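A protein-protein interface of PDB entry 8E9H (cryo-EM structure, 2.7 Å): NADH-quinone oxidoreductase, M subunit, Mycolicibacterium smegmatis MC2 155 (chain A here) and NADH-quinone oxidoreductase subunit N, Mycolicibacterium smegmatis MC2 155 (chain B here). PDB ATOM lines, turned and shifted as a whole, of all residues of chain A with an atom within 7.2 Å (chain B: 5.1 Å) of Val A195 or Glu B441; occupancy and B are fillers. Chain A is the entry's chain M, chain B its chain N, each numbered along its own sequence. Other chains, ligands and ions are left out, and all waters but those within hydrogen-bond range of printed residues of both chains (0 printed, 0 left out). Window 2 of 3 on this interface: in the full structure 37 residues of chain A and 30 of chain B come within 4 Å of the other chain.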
ATOM      1  N   SER A  73      19.919  -3.203  -0.012  1.00  0.00           N
ATOM      2  CA  SER A  73      19.011  -3.444  -1.126  1.00  0.00           C
ATOM      3  C   SER A  73      17.768  -2.571  -1.034  1.00  0.00           C
ATOM      4  O   SER A  73      17.257  -2.109  -2.060  1.00  0.00           O
ATOM      5  CB  SER A  73      18.617  -4.918  -1.166  1.00  0.00           C
ATOM      6  OG  SER A  73      17.776  -5.190  -2.273  1.00  0.00           O
ATOM      7  N   ALA A 189       2.831   4.836   2.059  1.00  0.00           N
ATOM      8  CA  ALA A 189       3.549   6.095   1.909  1.00  0.00           C
ATOM      9  C   ALA A 189       5.056   5.900   1.991  1.00  0.00           C
ATOM     10  O   ALA A 189       5.809   6.642   1.365  1.00  0.00           O
ATOM     11  CB  ALA A 189       3.092   7.085   2.976  1.00  0.00           C
ATOM     12  N   VAL A 190       5.510   4.923   2.768  1.00  0.00           N
ATOM     13  CA  VAL A 190       6.939   4.663   2.891  1.00  0.00           C
ATOM     14  C   VAL A 190       7.489   4.166   1.565  1.00  0.00           C
ATOM     15  O   VAL A 190       8.557   4.597   1.110  1.00  0.00           O
ATOM     16  CB  VAL A 190       7.199   3.658   4.028  1.00  0.00           C
ATOM     17  CG1 VAL A 190       8.639   3.198   4.016  1.00  0.00           C
ATOM     18  CG2 VAL A 190       6.853   4.278   5.363  1.00  0.00           C
ATOM     19  N   ILE A 191       6.763   3.260   0.917  1.00  0.00           N
ATOM     20  CA  ILE A 191       7.182   2.788  -0.395  1.00  0.00           C
ATOM     21  C   ILE A 191       7.094   3.915  -1.414  1.00  0.00           C
ATOM     22  O   ILE A 191       7.945   4.034  -2.302  1.00  0.00           O
ATOM     23  CB  ILE A 191       6.343   1.569  -0.809  1.00  0.00           C
ATOM     24  CG1 ILE A 191       6.770   0.363   0.024  1.00  0.00           C
ATOM     25  CG2 ILE A 191       6.499   1.299  -2.296  1.00  0.00           C
ATOM     26  CD1 ILE A 191       5.965  -0.868  -0.223  1.00  0.00           C
ATOM     27  N   GLY A 192       6.071   4.761  -1.304  1.00  0.00           N
ATOM     28  CA  GLY A 192       6.005   5.925  -2.171  1.00  0.00           C
ATOM     29  C   GLY A 192       7.201   6.839  -1.988  1.00  0.00           C
ATOM     30  O   GLY A 192       7.746   7.367  -2.957  1.00  0.00           O
ATOM     31  N   LEU A 193       7.620   7.038  -0.740  1.00  0.00           N
ATOM     32  CA  LEU A 193       8.797   7.849  -0.462  1.00  0.00           C
ATOM     33  C   LEU A 193      10.041   7.227  -1.069  1.00  0.00           C
ATOM     34  O   LEU A 193      10.879   7.930  -1.641  1.00  0.00           O
ATOM     35  CB  LEU A 193       8.970   8.012   1.046  1.00  0.00           C
ATOM     36  CG  LEU A 193      10.206   8.781   1.504  1.00  0.00           C
ATOM     37  CD1 LEU A 193      10.107  10.238   1.099  1.00  0.00           C
ATOM     38  CD2 LEU A 193      10.382   8.647   3.003  1.00  0.00           C
ATOM     39  N   TYR A 194      10.189   5.910  -0.940  1.00  0.00           N
ATOM     40  CA  TYR A 194      11.327   5.245  -1.559  1.00  0.00           C
ATOM     41  C   TYR A 194      11.322   5.464  -3.064  1.00  0.00           C
ATOM     42  O   TYR A 194      12.357   5.769  -3.665  1.00  0.00           O
ATOM     43  CB  TYR A 194      11.307   3.754  -1.240  1.00  0.00           C
ATOM     44  CG  TYR A 194      12.460   2.996  -1.849  1.00  0.00           C
ATOM     45  CD1 TYR A 194      12.379   2.491  -3.137  1.00  0.00           C
ATOM     46  CD2 TYR A 194      13.629   2.786  -1.139  1.00  0.00           C
ATOM     47  CE1 TYR A 194      13.428   1.803  -3.701  1.00  0.00           C
ATOM     48  CE2 TYR A 194      14.684   2.095  -1.694  1.00  0.00           C
ATOM     49  CZ  TYR A 194      14.578   1.606  -2.975  1.00  0.00           C
ATOM     50  OH  TYR A 194      15.626   0.916  -3.534  1.00  0.00           O
ATOM     51  N   VAL A 195      10.154   5.317  -3.688  1.00  0.00           N
ATOM     52  CA  VAL A 195      10.058   5.499  -5.132  1.00  0.00           C
ATOM     53  C   VAL A 195      10.430   6.923  -5.512  1.00  0.00           C
ATOM     54  O   VAL A 195      11.183   7.151  -6.466  1.00  0.00           O
ATOM     55  CB  VAL A 195       8.644   5.138  -5.618  1.00  0.00           C
ATOM     56  CG1 VAL A 195       8.432   5.625  -7.038  1.00  0.00           C
ATOM     57  CG2 VAL A 195       8.426   3.642  -5.528  1.00  0.00           C
ATOM     58  N   VAL A 196       9.911   7.903  -4.775  1.00  0.00           N
ATOM     59  CA  VAL A 196      10.183   9.296  -5.104  1.00  0.00           C
ATOM     60  C   VAL A 196      11.666   9.599  -4.950  1.00  0.00           C
ATOM     61  O   VAL A 196      12.271  10.251  -5.808  1.00  0.00           O
ATOM     62  CB  VAL A 196       9.319  10.226  -4.236  1.00  0.00           C
ATOM     63  CG1 VAL A 196       9.676  11.672  -4.498  1.00  0.00           C
ATOM     64  CG2 VAL A 196       7.848   9.997  -4.518  1.00  0.00           C
ATOM     65  N   THR A 197      12.277   9.133  -3.861  1.00  0.00           N
ATOM     66  CA  THR A 197      13.701   9.373  -3.662  1.00  0.00           C
ATOM     67  C   THR A 197      14.520   8.723  -4.765  1.00  0.00           C
ATOM     68  O   THR A 197      15.463   9.328  -5.286  1.00  0.00           O
ATOM     69  CB  THR A 197      14.142   8.845  -2.300  1.00  0.00           C
ATOM     70  OG1 THR A 197      13.807   7.458  -2.192  1.00  0.00           O
ATOM     71  CG2 THR A 197      13.469   9.619  -1.184  1.00  0.00           C
ATOM     72  N   ALA A 198      14.175   7.491  -5.139  1.00  0.00           N
ATOM     73  CA  ALA A 198      14.898   6.829  -6.216  1.00  0.00           C
ATOM     74  C   ALA A 198      14.774   7.615  -7.512  1.00  0.00           C
ATOM     75  O   ALA A 198      15.744   7.744  -8.266  1.00  0.00           O
ATOM     76  CB  ALA A 198      14.378   5.406  -6.399  1.00  0.00           C
ATOM     77  N   GLY A 199      13.591   8.156  -7.783  1.00  0.00           N
ATOM     78  CA  GLY A 199      13.366   8.928  -8.987  1.00  0.00           C
ATOM     79  C   GLY A 199      13.947  10.322  -8.968  1.00  0.00           C
ATOM     80  O   GLY A 199      13.776  11.056  -9.945  1.00  0.00           O
ATOM     81  N   SER A 200      14.623  10.709  -7.891  1.00  0.00           N
ATOM     82  CA  SER A 200      15.237  12.022  -7.773  1.00  0.00           C
ATOM     83  C   SER A 200      16.750  11.880  -7.772  1.00  0.00           C
ATOM     84  O   SER A 200      17.297  10.949  -7.173  1.00  0.00           O
ATOM     85  CB  SER A 200      14.785  12.733  -6.498  1.00  0.00           C
ATOM     86  OG  SER A 200      15.346  14.031  -6.421  1.00  0.00           O
ATOM     87  N   GLY A 206      17.130   4.910  -4.149  1.00  0.00           N
ATOM     88  CA  GLY A 206      16.089   4.959  -3.147  1.00  0.00           C
ATOM     89  C   GLY A 206      16.709   4.930  -1.767  1.00  0.00           C
ATOM     90  O   GLY A 206      17.572   4.092  -1.490  1.00  0.00           O
ATOM     91  N   THR A 207      16.292   5.845  -0.898  1.00  0.00           N
ATOM     92  CA  THR A 207      16.964   6.031   0.378  1.00  0.00           C
ATOM     93  C   THR A 207      15.933   6.116   1.491  1.00  0.00           C
ATOM     94  O   THR A 207      14.816   6.597   1.288  1.00  0.00           O
ATOM     95  CB  THR A 207      17.831   7.295   0.361  1.00  0.00           C
ATOM     96  OG1 THR A 207      18.882   7.141  -0.600  1.00  0.00           O
ATOM     97  CG2 THR A 207      18.437   7.551   1.722  1.00  0.00           C
ATOM     98  N   PHE A 208      16.324   5.636   2.672  1.00  0.00           N
ATOM     99  CA  PHE A 208      15.510   5.756   3.873  1.00  0.00           C
ATOM    100  C   PHE A 208      16.248   6.471   4.995  1.00  0.00           C
ATOM    101  O   PHE A 208      15.700   6.602   6.093  1.00  0.00           O
ATOM    102  CB  PHE A 208      15.059   4.377   4.362  1.00  0.00           C
ATOM    103  CG  PHE A 208      13.930   3.791   3.570  1.00  0.00           C
ATOM    104  CD1 PHE A 208      12.721   4.449   3.470  1.00  0.00           C
ATOM    105  CD2 PHE A 208      14.076   2.573   2.936  1.00  0.00           C
ATOM    106  CE1 PHE A 208      11.686   3.910   2.747  1.00  0.00           C
ATOM    107  CE2 PHE A 208      13.042   2.029   2.214  1.00  0.00           C
ATOM    108  CZ  PHE A 208      11.845   2.697   2.122  1.00  0.00           C
ATOM    109  N   PHE A 222      15.865  18.138  -3.216  1.00  0.00           N
ATOM    110  CA  PHE A 222      14.901  17.050  -3.367  1.00  0.00           C
ATOM    111  C   PHE A 222      13.485  17.607  -3.521  1.00  0.00           C
ATOM    112  O   PHE A 222      12.587  17.360  -2.719  1.00  0.00           O
ATOM    113  CB  PHE A 222      15.003  16.098  -2.179  1.00  0.00           C
ATOM    114  CG  PHE A 222      14.046  14.943  -2.234  1.00  0.00           C
ATOM    115  CD1 PHE A 222      13.607  14.437  -3.442  1.00  0.00           C
ATOM    116  CD2 PHE A 222      13.594  14.357  -1.068  1.00  0.00           C
ATOM    117  CE1 PHE A 222      12.732  13.376  -3.483  1.00  0.00           C
ATOM    118  CE2 PHE A 222      12.720  13.296  -1.104  1.00  0.00           C
ATOM    119  CZ  PHE A 222      12.289  12.804  -2.311  1.00  0.00           C
ATOM    120  N   ASN B 357      10.630  -5.110 -13.771  1.00  0.00           N
ATOM    121  CA  ASN B 357      11.953  -4.549 -13.567  1.00  0.00           C
ATOM    122  C   ASN B 357      12.784  -5.548 -12.780  1.00  0.00           C
ATOM    123  O   ASN B 357      12.232  -6.398 -12.073  1.00  0.00           O
ATOM    124  CB  ASN B 357      11.887  -3.207 -12.826  1.00  0.00           C
ATOM    125  CG  ASN B 357      11.114  -3.295 -11.532  1.00  0.00           C
ATOM    126  OD1 ASN B 357      11.071  -4.343 -10.893  1.00  0.00           O
ATOM    127  ND2 ASN B 357      10.498  -2.191 -11.137  1.00  0.00           N
ATOM    128  N   ALA B 359      14.326  -5.321 -10.068  1.00  0.00           N
ATOM    129  CA  ALA B 359      13.834  -5.324  -8.699  1.00  0.00           C
ATOM    130  C   ALA B 359      12.631  -6.239  -8.564  1.00  0.00           C
ATOM    131  O   ALA B 359      12.477  -6.910  -7.541  1.00  0.00           O
ATOM    132  CB  ALA B 359      13.475  -3.905  -8.263  1.00  0.00           C
ATOM    133  N   PHE B 436       6.240  -4.989  -3.037  1.00  0.00           N
ATOM    134  CA  PHE B 436       5.560  -3.710  -3.205  1.00  0.00           C
ATOM    135  C   PHE B 436       6.518  -2.613  -3.641  1.00  0.00           C
ATOM    136  O   PHE B 436       6.134  -1.738  -4.419  1.00  0.00           O
ATOM    137  CB  PHE B 436       4.861  -3.307  -1.906  1.00  0.00           C
ATOM    138  CG  PHE B 436       3.635  -4.118  -1.584  1.00  0.00           C
ATOM    139  CD1 PHE B 436       3.031  -4.923  -2.534  1.00  0.00           C
ATOM    140  CD2 PHE B 436       3.085  -4.064  -0.320  1.00  0.00           C
ATOM    141  CE1 PHE B 436       1.911  -5.656  -2.223  1.00  0.00           C
ATOM    142  CE2 PHE B 436       1.963  -4.797  -0.008  1.00  0.00           C
ATOM    143  CZ  PHE B 436       1.376  -5.592  -0.961  1.00  0.00           C
ATOM    144  N   LYS B 437       7.756  -2.629  -3.150  1.00  0.00           N
ATOM    145  CA  LYS B 437       8.755  -1.677  -3.614  1.00  0.00           C
ATOM    146  C   LYS B 437       9.040  -1.878  -5.091  1.00  0.00           C
ATOM    147  O   LYS B 437       9.145  -0.912  -5.856  1.00  0.00           O
ATOM    148  CB  LYS B 437      10.032  -1.840  -2.794  1.00  0.00           C
ATOM    149  CG  LYS B 437      11.163  -0.912  -3.183  1.00  0.00           C
ATOM    150  CD  LYS B 437      12.469  -1.384  -2.580  1.00  0.00           C
ATOM    151  CE  LYS B 437      13.063  -2.532  -3.377  1.00  0.00           C
ATOM    152  NZ  LYS B 437      13.903  -2.044  -4.502  1.00  0.00           N
ATOM    153  N   ALA B 438       9.171  -3.135  -5.515  1.00  0.00           N
ATOM    154  CA  ALA B 438       9.384  -3.397  -6.931  1.00  0.00           C
ATOM    155  C   ALA B 438       8.216  -2.881  -7.755  1.00  0.00           C
ATOM    156  O   ALA B 438       8.412  -2.274  -8.814  1.00  0.00           O
ATOM    157  CB  ALA B 438       9.584  -4.890  -7.163  1.00  0.00           C
ATOM    158  N   ALA B 439       6.991  -3.106  -7.283  1.00  0.00           N
ATOM    159  CA  ALA B 439       5.826  -2.609  -8.004  1.00  0.00           C
ATOM    160  C   ALA B 439       5.827  -1.089  -8.069  1.00  0.00           C
ATOM    161  O   ALA B 439       5.536  -0.503  -9.117  1.00  0.00           O
ATOM    162  CB  ALA B 439       4.546  -3.114  -7.342  1.00  0.00           C
ATOM    163  N   GLY B 440       6.153  -0.432  -6.956  1.00  0.00           N
ATOM    164  CA  GLY B 440       6.173   1.021  -6.947  1.00  0.00           C
ATOM    165  C   GLY B 440       7.192   1.586  -7.915  1.00  0.00           C
ATOM    166  O   GLY B 440       6.902   2.516  -8.669  1.00  0.00           O
ATOM    167  N   GLU B 441       8.399   1.022  -7.914  1.00  0.00           N
ATOM    168  CA  GLU B 441       9.405   1.460  -8.874  1.00  0.00           C
ATOM    169  C   GLU B 441       8.939   1.229 -10.303  1.00  0.00           C
ATOM    170  O   GLU B 441       9.378   1.931 -11.220  1.00  0.00           O
ATOM    171  CB  GLU B 441      10.720   0.729  -8.629  1.00  0.00           C
ATOM    172  CG  GLU B 441      11.405   1.117  -7.339  1.00  0.00           C
ATOM    173  CD  GLU B 441      12.691   0.354  -7.120  1.00  0.00           C
ATOM    174  OE1 GLU B 441      13.711   0.717  -7.739  1.00  0.00           O
ATOM    175  OE2 GLU B 441      12.683  -0.613  -6.331  1.00  0.00           O
ATOM    176  N   GLY B 442       8.057   0.261 -10.511  1.00  0.00           N
ATOM    177  CA  GLY B 442       7.531  -0.047 -11.820  1.00  0.00           C
ATOM    178  C   GLY B 442       6.325   0.761 -12.228  1.00  0.00           C
ATOM    179  O   GLY B 442       5.715   0.465 -13.257  1.00  0.00           O
ATOM    180  N   GLY B 443       5.952   1.772 -11.449  1.00  0.00           N
ATOM    181  CA  GLY B 443       4.809   2.594 -11.773  1.00  0.00           C
ATOM    182  C   GLY B 443       3.472   2.002 -11.398  1.00  0.00           C
ATOM    183  O   GLY B 443       2.440   2.530 -11.828  1.00  0.00           O
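Hydrophobic or aromatic side chains of chain A that line the printed part of chain B: Ile A191, Tyr A194 and Val A195.
Of chain B, only Gly B440 and Glu B441 come within 4 Å of Val A195.
Of chain A, only Tyr A194 (3.6 Å) and Val A195 (3.5 Å) come within 4 Å of Glu B441.
Of the printed residues of chain A, Gly B440 touches Val A195 (3.4 Å).
Of the printed residues of chain B, Ile A191 touches Phe B436 and Lys B437.
Printed residues of chain A within 4 Å of Phe B436: Ile A191.
Ala B438 touches none of the printed residues of chain A.
The nearest residue of chain A that does not touch Glu B441 is Ala A198 (4.9 Å).
Phe B436 touches Ile A191 (CB to CD1, 3.2 Å).
Lys B437 touches Ile A191 (N to CD1, 3.9 Å).
Tyr A194 touches Lys B437 (CE1 to CD, 3.5 Å).
Tyr A194 touches Glu B441.
C of Gly B440 touches CG2 of Val A195, at 3.4 Å.
Glu B441 touches Val A195.
The side-chain carboxylate of Glu B441 is in salt-bridge range of the side-chain amino group of Lys B437 (2.6 Å).
OG1 of Thr A197 sits at hydrogen-bond distance from O of Tyr A194, 2.7 Å away.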
